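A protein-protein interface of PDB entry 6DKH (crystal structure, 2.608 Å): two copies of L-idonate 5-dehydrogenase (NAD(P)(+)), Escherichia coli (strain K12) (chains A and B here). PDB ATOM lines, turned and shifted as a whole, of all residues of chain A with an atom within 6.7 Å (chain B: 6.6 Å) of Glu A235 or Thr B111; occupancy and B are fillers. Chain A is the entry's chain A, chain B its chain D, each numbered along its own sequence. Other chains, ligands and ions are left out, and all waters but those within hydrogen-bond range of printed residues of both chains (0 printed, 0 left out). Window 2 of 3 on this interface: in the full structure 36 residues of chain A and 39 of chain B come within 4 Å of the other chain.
Of the 13 printed residues of chain B, 5 touch a printed residue of chain A.
Among the printed residues, no Asp or Glu carboxylate lies within 4 Å of a Lys or Arg side-chain nitrogen of the other chain.
The side-chain sulfur (SG) of Cys B110 sits close to the backbone NH (N) of Met B113 (3.7 Å).
The side-chain sulfur (SG) of Cys B110 lies close to the backbone NH (N) of Asp B112 (3.3 Å).
NZ of Lys A285 sits at hydrogen-bond distance from O of Thr A259 (2.8 Å).
O of Lys A236 lies within hydrogen-bond range of NZ of Lys A285.
N of Ala A261 is in hydrogen-bond range of O of Lys A236 (3.4 Å).
SG of Cys B99 sits close to N of Tyr B101, at 3.5 Å.
Among the printed residues, pairs that only touch across the chains: Glu A235 with Thr B111, Lys A236 with Gln B109, Lys A236 with Cys B110, Gly A237 with Tyr B101, Arg A260 with Lys B100, Arg A260 with Tyr B101, Ala A261 with Gln B109 and Lys A285 with Gln B109.
O of Glu A235 is in hydrogen-bond range of OH of Tyr B101, at 2.9 Å.
OH of Tyr B101 sits at hydrogen-bond distance from N of Ala A261 (3.0 Å).
The side-chain hydroxyl of Tyr B101 sits at hydrogen-bond distance from the backbone carbonyl oxygen of Lys A236, 3.3 Å away.
The backbone carbonyl oxygen of Glu A235 lies close to the side-chain amino group of Lys B100 (3.4 Å).
The side-chain amino group (NZ) of Lys B100 is in hydrogen-bond range of the backbone carbonyl oxygen (O) of Gly A237 (2.7 Å).
No position is printed for both chains.
Of chain B, only Lys B100 (3.2 Å), Tyr B101 (2.9 Å) and Thr B111 (3.6 Å) come within 4 Å of Glu A235.
Of the printed residues of chain B, Ala A261 touches Tyr B101 and Gln B109.
Of the printed residues of chain B, Lys A285 touches Gln B109 (3.4 Å).
Cys B96 touches none of the printed residues of chain A.
Of the printed residues of chain A, Gln B109 touches Lys A236 (3.5 Å), Ala A261 (3.7 Å) and Lys A285 (3.4 Å).
Of the printed residues of chain A, Cys B110 touches Lys A236.
Of chain A, only Glu A235 comes within 4 Å of Thr B111.
The nearest printed residue of chain A that does not touch Gln B109 is Glu A235 (6.6 Å).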
ATOM      1  N   ASP A 230      12.795  -6.055  -7.655  1.00  0.00           N
ATOM      2  CA  ASP A 230      12.558  -4.975  -8.609  1.00  0.00           C
ATOM      3  C   ASP A 230      12.405  -3.627  -7.916  1.00  0.00           C
ATOM      4  O   ASP A 230      12.797  -2.599  -8.479  1.00  0.00           O
ATOM      5  CB  ASP A 230      11.318  -5.276  -9.452  1.00  0.00           C
ATOM      6  CG  ASP A 230      11.598  -6.256 -10.574  1.00  0.00           C
ATOM      7  OD1 ASP A 230      12.783  -6.568 -10.810  1.00  0.00           O
ATOM      8  OD2 ASP A 230      10.630  -6.712 -11.217  1.00  0.00           O
ATOM      9  N   HIS A 231      11.833  -3.609  -6.709  1.00  0.00           N
ATOM     10  CA  HIS A 231      11.601  -2.340  -6.026  1.00  0.00           C
ATOM     11  C   HIS A 231      12.910  -1.628  -5.716  1.00  0.00           C
ATOM     12  O   HIS A 231      13.001  -0.401  -5.838  1.00  0.00           O
ATOM     13  CB  HIS A 231      10.802  -2.569  -4.743  1.00  0.00           C
ATOM     14  CG  HIS A 231      10.866  -1.423  -3.780  1.00  0.00           C
ATOM     15  ND1 HIS A 231      10.604  -0.120  -4.150  1.00  0.00           N
ATOM     16  CD2 HIS A 231      11.162  -1.385  -2.459  1.00  0.00           C
ATOM     17  CE1 HIS A 231      10.737   0.671  -3.099  1.00  0.00           C
ATOM     18  NE2 HIS A 231      11.075  -0.073  -2.060  1.00  0.00           N
ATOM     19  N   TRP A 232      13.940  -2.377  -5.324  1.00  0.00           N
ATOM     20  CA  TRP A 232      15.216  -1.769  -4.972  1.00  0.00           C
ATOM     21  C   TRP A 232      16.105  -1.502  -6.178  1.00  0.00           C
ATOM     22  O   TRP A 232      17.161  -0.882  -6.019  1.00  0.00           O
ATOM     23  CB  TRP A 232      15.959  -2.651  -3.967  1.00  0.00           C
ATOM     24  CG  TRP A 232      15.281  -2.719  -2.635  1.00  0.00           C
ATOM     25  CD1 TRP A 232      14.996  -1.672  -1.808  1.00  0.00           C
ATOM     26  CD2 TRP A 232      14.804  -3.895  -1.971  1.00  0.00           C
ATOM     27  NE1 TRP A 232      14.370  -2.121  -0.672  1.00  0.00           N
ATOM     28  CE2 TRP A 232      14.240  -3.483  -0.746  1.00  0.00           C
ATOM     29  CE3 TRP A 232      14.798  -5.256  -2.291  1.00  0.00           C
ATOM     30  CZ2 TRP A 232      13.677  -4.380   0.157  1.00  0.00           C
ATOM     31  CZ3 TRP A 232      14.238  -6.145  -1.394  1.00  0.00           C
ATOM     32  CH2 TRP A 232      13.684  -5.703  -0.184  1.00  0.00           C
ATOM     33  N   LYS A 233      15.710  -1.943  -7.372  1.00  0.00           N
ATOM     34  CA  LYS A 233      16.470  -1.670  -8.583  1.00  0.00           C
ATOM     35  C   LYS A 233      15.881  -0.538  -9.412  1.00  0.00           C
ATOM     36  O   LYS A 233      16.535  -0.080 -10.355  1.00  0.00           O
ATOM     37  CB  LYS A 233      16.570  -2.933  -9.448  1.00  0.00           C
ATOM     38  CG  LYS A 233      17.258  -4.101  -8.763  1.00  0.00           C
ATOM     39  CD  LYS A 233      17.443  -5.272  -9.714  1.00  0.00           C
ATOM     40  CE  LYS A 233      18.062  -6.465  -9.004  1.00  0.00           C
ATOM     41  NZ  LYS A 233      18.421  -7.554  -9.956  1.00  0.00           N
ATOM     42  N   ALA A 234      14.677  -0.078  -9.089  1.00  0.00           N
ATOM     43  CA  ALA A 234      14.052   0.994  -9.847  1.00  0.00           C
ATOM     44  C   ALA A 234      14.811   2.303  -9.661  1.00  0.00           C
ATOM     45  O   ALA A 234      15.433   2.547  -8.623  1.00  0.00           O
ATOM     46  CB  ALA A 234      12.595   1.170  -9.425  1.00  0.00           C
ATOM     47  N   GLU A 235      14.751   3.148 -10.694  1.00  0.00           N
ATOM     48  CA  GLU A 235      15.426   4.447 -10.702  1.00  0.00           C
ATOM     49  C   GLU A 235      16.928   4.293 -10.470  1.00  0.00           C
ATOM     50  O   GLU A 235      17.530   5.023  -9.679  1.00  0.00           O
ATOM     51  CB  GLU A 235      14.803   5.401  -9.681  1.00  0.00           C
ATOM     52  CG  GLU A 235      13.323   5.690  -9.915  1.00  0.00           C
ATOM     53  CD  GLU A 235      13.052   6.372 -11.248  1.00  0.00           C
ATOM     54  OE1 GLU A 235      12.989   5.674 -12.283  1.00  0.00           O
ATOM     55  OE2 GLU A 235      12.903   7.612 -11.260  1.00  0.00           O
ATOM     56  N   LYS A 236      17.529   3.322 -11.161  1.00  0.00           N
ATOM     57  CA  LYS A 236      18.975   3.091 -11.137  1.00  0.00           C
ATOM     58  C   LYS A 236      19.496   2.772  -9.737  1.00  0.00           C
ATOM     59  O   LYS A 236      20.652   3.057  -9.420  1.00  0.00           O
ATOM     60  CB  LYS A 236      19.745   4.281 -11.724  1.00  0.00           C
ATOM     61  CG  LYS A 236      19.677   4.409 -13.238  1.00  0.00           C
ATOM     62  CD  LYS A 236      20.961   5.035 -13.770  1.00  0.00           C
ATOM     63  CE  LYS A 236      20.722   6.396 -14.402  1.00  0.00           C
ATOM     64  NZ  LYS A 236      20.388   6.284 -15.849  1.00  0.00           N
ATOM     65  N   GLY A 237      18.666   2.177  -8.885  1.00  0.00           N
ATOM     66  CA  GLY A 237      19.115   1.769  -7.568  1.00  0.00           C
ATOM     67  C   GLY A 237      18.449   2.507  -6.422  1.00  0.00           C
ATOM     68  O   GLY A 237      17.893   3.593  -6.604  1.00  0.00           O
ATOM     69  N   TYR A 238      18.517   1.929  -5.227  1.00  0.00           N
ATOM     70  CA  TYR A 238      17.815   2.448  -4.056  1.00  0.00           C
ATOM     71  C   TYR A 238      18.729   2.786  -2.890  1.00  0.00           C
ATOM     72  O   TYR A 238      18.545   3.826  -2.248  1.00  0.00           O
ATOM     73  CB  TYR A 238      16.755   1.435  -3.589  1.00  0.00           C
ATOM     74  CG  TYR A 238      16.059   1.787  -2.291  1.00  0.00           C
ATOM     75  CD1 TYR A 238      14.967   2.644  -2.276  1.00  0.00           C
ATOM     76  CD2 TYR A 238      16.483   1.246  -1.085  1.00  0.00           C
ATOM     77  CE1 TYR A 238      14.322   2.961  -1.091  1.00  0.00           C
ATOM     78  CE2 TYR A 238      15.847   1.555   0.103  1.00  0.00           C
ATOM     79  CZ  TYR A 238      14.767   2.413   0.095  1.00  0.00           C
ATOM     80  OH  TYR A 238      14.134   2.720   1.277  1.00  0.00           O
ATOM     81  N   THR A 259      22.443  -0.628  -5.718  1.00  0.00           N
ATOM     82  CA  THR A 259      23.035   0.636  -5.305  1.00  0.00           C
ATOM     83  C   THR A 259      22.664   1.732  -6.295  1.00  0.00           C
ATOM     84  O   THR A 259      22.749   1.542  -7.514  1.00  0.00           O
ATOM     85  CB  THR A 259      24.553   0.514  -5.206  1.00  0.00           C
ATOM     86  OG1 THR A 259      24.885  -0.584  -4.353  1.00  0.00           O
ATOM     87  CG2 THR A 259      25.153   1.784  -4.633  1.00  0.00           C
ATOM     88  N   ARG A 260      22.241   2.878  -5.772  1.00  0.00           N
ATOM     89  CA  ARG A 260      21.884   3.991  -6.633  1.00  0.00           C
ATOM     90  C   ARG A 260      23.128   4.585  -7.284  1.00  0.00           C
ATOM     91  O   ARG A 260      24.263   4.341  -6.862  1.00  0.00           O
ATOM     92  CB  ARG A 260      21.125   5.063  -5.851  1.00  0.00           C
ATOM     93  CG  ARG A 260      21.769   5.478  -4.547  1.00  0.00           C
ATOM     94  CD  ARG A 260      21.014   6.641  -3.939  1.00  0.00           C
ATOM     95  NE  ARG A 260      21.580   7.917  -4.362  1.00  0.00           N
ATOM     96  CZ  ARG A 260      20.906   9.058  -4.415  1.00  0.00           C
ATOM     97  NH1 ARG A 260      19.621   9.094  -4.086  1.00  0.00           N
ATOM     98  NH2 ARG A 260      21.518  10.165  -4.809  1.00  0.00           N
ATOM     99  N   ALA A 261      22.898   5.363  -8.339  1.00  0.00           N
ATOM    100  CA  ALA A 261      23.995   5.960  -9.087  1.00  0.00           C
ATOM    101  C   ALA A 261      24.825   6.852  -8.178  1.00  0.00           C
ATOM    102  O   ALA A 261      24.293   7.540  -7.300  1.00  0.00           O
ATOM    103  CB  ALA A 261      23.457   6.764 -10.270  1.00  0.00           C
ATOM    104  N   LYS A 285      26.787   4.325 -14.025  1.00  0.00           N
ATOM    105  CA  LYS A 285      26.209   4.826 -12.786  1.00  0.00           C
ATOM    106  C   LYS A 285      27.236   5.474 -11.867  1.00  0.00           C
ATOM    107  O   LYS A 285      26.845   6.101 -10.875  1.00  0.00           O
ATOM    108  CB  LYS A 285      25.501   3.687 -12.045  1.00  0.00           C
ATOM    109  CG  LYS A 285      24.477   2.953 -12.896  1.00  0.00           C
ATOM    110  CD  LYS A 285      23.960   1.708 -12.197  1.00  0.00           C
ATOM    111  CE  LYS A 285      23.319   2.048 -10.866  1.00  0.00           C
ATOM    112  NZ  LYS A 285      22.733   0.844 -10.217  1.00  0.00           N
ATOM    113  N   CYS B  96      15.548  16.100 -17.178  1.00  0.00           N
ATOM    114  CA  CYS B  96      14.361  16.576 -16.491  1.00  0.00           C
ATOM    115  C   CYS B  96      14.762  17.267 -15.191  1.00  0.00           C
ATOM    116  O   CYS B  96      15.883  17.117 -14.698  1.00  0.00           O
ATOM    117  CB  CYS B  96      13.394  15.426 -16.204  1.00  0.00           C
ATOM    118  SG  CYS B  96      13.937  14.282 -14.913  1.00  0.00           S
ATOM    119  N   CYS B  99      13.549  14.405 -11.255  1.00  0.00           N
ATOM    120  CA  CYS B  99      13.991  13.103 -10.780  1.00  0.00           C
ATOM    121  C   CYS B  99      14.962  13.272  -9.611  1.00  0.00           C
ATOM    122  O   CYS B  99      15.465  14.365  -9.340  1.00  0.00           O
ATOM    123  CB  CYS B  99      14.638  12.302 -11.910  1.00  0.00           C
ATOM    124  SG  CYS B  99      16.400  12.611 -12.147  1.00  0.00           S
ATOM    125  N   LYS B 100      15.227  12.165  -8.911  1.00  0.00           N
ATOM    126  CA  LYS B 100      16.011  12.254  -7.684  1.00  0.00           C
ATOM    127  C   LYS B 100      17.463  12.633  -7.954  1.00  0.00           C
ATOM    128  O   LYS B 100      18.086  13.309  -7.129  1.00  0.00           O
ATOM    129  CB  LYS B 100      15.941  10.939  -6.906  1.00  0.00           C
ATOM    130  CG  LYS B 100      16.503   9.728  -7.633  1.00  0.00           C
ATOM    131  CD  LYS B 100      16.666   8.564  -6.668  1.00  0.00           C
ATOM    132  CE  LYS B 100      16.951   7.264  -7.400  1.00  0.00           C
ATOM    133  NZ  LYS B 100      17.067   6.121  -6.452  1.00  0.00           N
ATOM    134  N   TYR B 101      18.019  12.220  -9.094  1.00  0.00           N
ATOM    135  CA  TYR B 101      19.407  12.555  -9.386  1.00  0.00           C
ATOM    136  C   TYR B 101      19.560  14.000  -9.846  1.00  0.00           C
ATOM    137  O   TYR B 101      20.566  14.643  -9.526  1.00  0.00           O
ATOM    138  CB  TYR B 101      19.973  11.599 -10.437  1.00  0.00           C
ATOM    139  CG  TYR B 101      19.986  10.155  -9.991  1.00  0.00           C
ATOM    140  CD1 TYR B 101      20.832   9.730  -8.975  1.00  0.00           C
ATOM    141  CD2 TYR B 101      19.150   9.217 -10.583  1.00  0.00           C
ATOM    142  CE1 TYR B 101      20.844   8.414  -8.562  1.00  0.00           C
ATOM    143  CE2 TYR B 101      19.159   7.897 -10.178  1.00  0.00           C
ATOM    144  CZ  TYR B 101      20.007   7.501  -9.167  1.00  0.00           C
ATOM    145  OH  TYR B 101      20.018   6.188  -8.760  1.00  0.00           O
ATOM    146  N   CYS B 102      18.582  14.527 -10.585  1.00  0.00           N
ATOM    147  CA  CYS B 102      18.641  15.921 -11.005  1.00  0.00           C
ATOM    148  C   CYS B 102      18.331  16.876  -9.861  1.00  0.00           C
ATOM    149  O   CYS B 102      18.830  18.007  -9.851  1.00  0.00           O
ATOM    150  CB  CYS B 102      17.679  16.160 -12.169  1.00  0.00           C
ATOM    151  SG  CYS B 102      18.148  15.301 -13.687  1.00  0.00           S
ATOM    152  N   GLU B 107      22.770  15.715 -12.689  1.00  0.00           N
ATOM    153  CA  GLU B 107      21.975  15.644 -13.911  1.00  0.00           C
ATOM    154  C   GLU B 107      22.529  14.651 -14.927  1.00  0.00           C
ATOM    155  O   GLU B 107      21.801  14.250 -15.840  1.00  0.00           O
ATOM    156  CB  GLU B 107      21.868  17.031 -14.556  1.00  0.00           C
ATOM    157  CG  GLU B 107      20.911  17.988 -13.852  1.00  0.00           C
ATOM    158  CD  GLU B 107      21.604  18.885 -12.843  1.00  0.00           C
ATOM    159  OE1 GLU B 107      22.832  18.746 -12.664  1.00  0.00           O
ATOM    160  OE2 GLU B 107      20.920  19.734 -12.231  1.00  0.00           O
ATOM    161  N   GLN B 109      23.136  11.609 -14.404  1.00  0.00           N
ATOM    162  CA  GLN B 109      22.507  10.323 -14.127  1.00  0.00           C
ATOM    163  C   GLN B 109      20.984  10.413 -14.167  1.00  0.00           C
ATOM    164  O   GLN B 109      20.297   9.712 -13.423  1.00  0.00           O
ATOM    165  CB  GLN B 109      22.967   9.786 -12.772  1.00  0.00           C
ATOM    166  CG  GLN B 109      24.458   9.504 -12.678  1.00  0.00           C
ATOM    167  CD  GLN B 109      24.869   8.265 -13.448  1.00  0.00           C
ATOM    168  OE1 GLN B 109      24.032   7.438 -13.811  1.00  0.00           O
ATOM    169  NE2 GLN B 109      26.166   8.131 -13.701  1.00  0.00           N
ATOM    170  N   CYS B 110      20.447  11.271 -15.033  1.00  0.00           N
ATOM    171  CA  CYS B 110      19.004  11.466 -15.095  1.00  0.00           C
ATOM    172  C   CYS B 110      18.304  10.196 -15.564  1.00  0.00           C
ATOM    173  O   CYS B 110      18.784   9.493 -16.457  1.00  0.00           O
ATOM    174  CB  CYS B 110      18.670  12.627 -16.031  1.00  0.00           C
ATOM    175  SG  CYS B 110      16.900  12.907 -16.273  1.00  0.00           S
ATOM    176  N   THR B 111      17.155   9.906 -14.949  1.00  0.00           N
ATOM    177  CA  THR B 111      16.391   8.722 -15.330  1.00  0.00           C
ATOM    178  C   THR B 111      15.705   8.905 -16.677  1.00  0.00           C
ATOM    179  O   THR B 111      15.576   7.942 -17.441  1.00  0.00           O
ATOM    180  CB  THR B 111      15.358   8.391 -14.252  1.00  0.00           C
ATOM    181  OG1 THR B 111      14.563   9.550 -13.977  1.00  0.00           O
ATOM    182  CG2 THR B 111      16.049   7.943 -12.973  1.00  0.00           C
ATOM    183  N   ASP B 112      15.259  10.122 -16.986  1.00  0.00           N
ATOM    184  CA  ASP B 112      14.637  10.401 -18.274  1.00  0.00           C
ATOM    185  C   ASP B 112      15.567  11.266 -19.116  1.00  0.00           C
ATOM    186  O   ASP B 112      15.167  12.319 -19.623  1.00  0.00           O
ATOM    187  CB  ASP B 112      13.280  11.078 -18.082  1.00  0.00           C
ATOM    188  CG  ASP B 112      12.379  10.933 -19.292  1.00  0.00           C
ATOM    189  OD1 ASP B 112      12.838  10.380 -20.313  1.00  0.00           O
ATOM    190  OD2 ASP B 112      11.209  11.364 -19.220  1.00  0.00           O
ATOM    191  N   MET B 113      16.810  10.818 -19.265  1.00  0.00           N
ATOM    192  CA  MET B 113      17.824  11.580 -19.978  1.00  0.00           C
ATOM    193  C   MET B 113      17.564  11.565 -21.481  1.00  0.00           C
ATOM    194  O   MET B 113      17.070  10.584 -22.042  1.00  0.00           O
ATOM    195  CB  MET B 113      19.211  11.011 -19.676  1.00  0.00           C
ATOM    196  CG  MET B 113      20.345  11.733 -20.370  1.00  0.00           C
ATOM    197  SD  MET B 113      20.342  13.489 -19.980  1.00  0.00           S
ATOM    198  CE  MET B 113      21.210  14.123 -21.403  1.00  0.00           C
ATOM    199  N   MET B 120      19.549   5.233 -27.097  1.00  0.00           N
ATOM    200  CA  MET B 120      19.204   4.509 -25.878  1.00  0.00           C
ATOM    201  C   MET B 120      17.704   4.261 -25.773  1.00  0.00           C
ATOM    202  O   MET B 120      17.274   3.132 -25.510  1.00  0.00           O
ATOM    203  CB  MET B 120      19.700   5.283 -24.658  1.00  0.00           C
ATOM    204  CG  MET B 120      19.335   4.651 -23.323  1.00  0.00           C
ATOM    205  SD  MET B 120      19.959   5.594 -21.918  1.00  0.00           S
ATOM    206  CE  MET B 120      19.192   4.723 -20.554  1.00  0.00           C
ATOM    207  N   TYR B 121      16.898   5.300 -25.961  1.00  0.00           N
ATOM    208  CA  TYR B 121      15.451   5.171 -25.962  1.00  0.00           C
ATOM    209  C   TYR B 121      14.935   5.188 -27.394  1.00  0.00           C
ATOM    210  O   TYR B 121      15.651   5.544 -28.332  1.00  0.00           O
ATOM    211  CB  TYR B 121      14.798   6.300 -25.158  1.00  0.00           C
ATOM    212  CG  TYR B 121      15.357   6.491 -23.764  1.00  0.00           C
ATOM    213  CD1 TYR B 121      14.843   5.787 -22.683  1.00  0.00           C
ATOM    214  CD2 TYR B 121      16.391   7.387 -23.528  1.00  0.00           C
ATOM    215  CE1 TYR B 121      15.350   5.965 -21.407  1.00  0.00           C
ATOM    216  CE2 TYR B 121      16.906   7.568 -22.260  1.00  0.00           C
ATOM    217  CZ  TYR B 121      16.381   6.858 -21.202  1.00  0.00           C
ATOM    218  OH  TYR B 121      16.894   7.043 -19.939  1.00  0.00           O
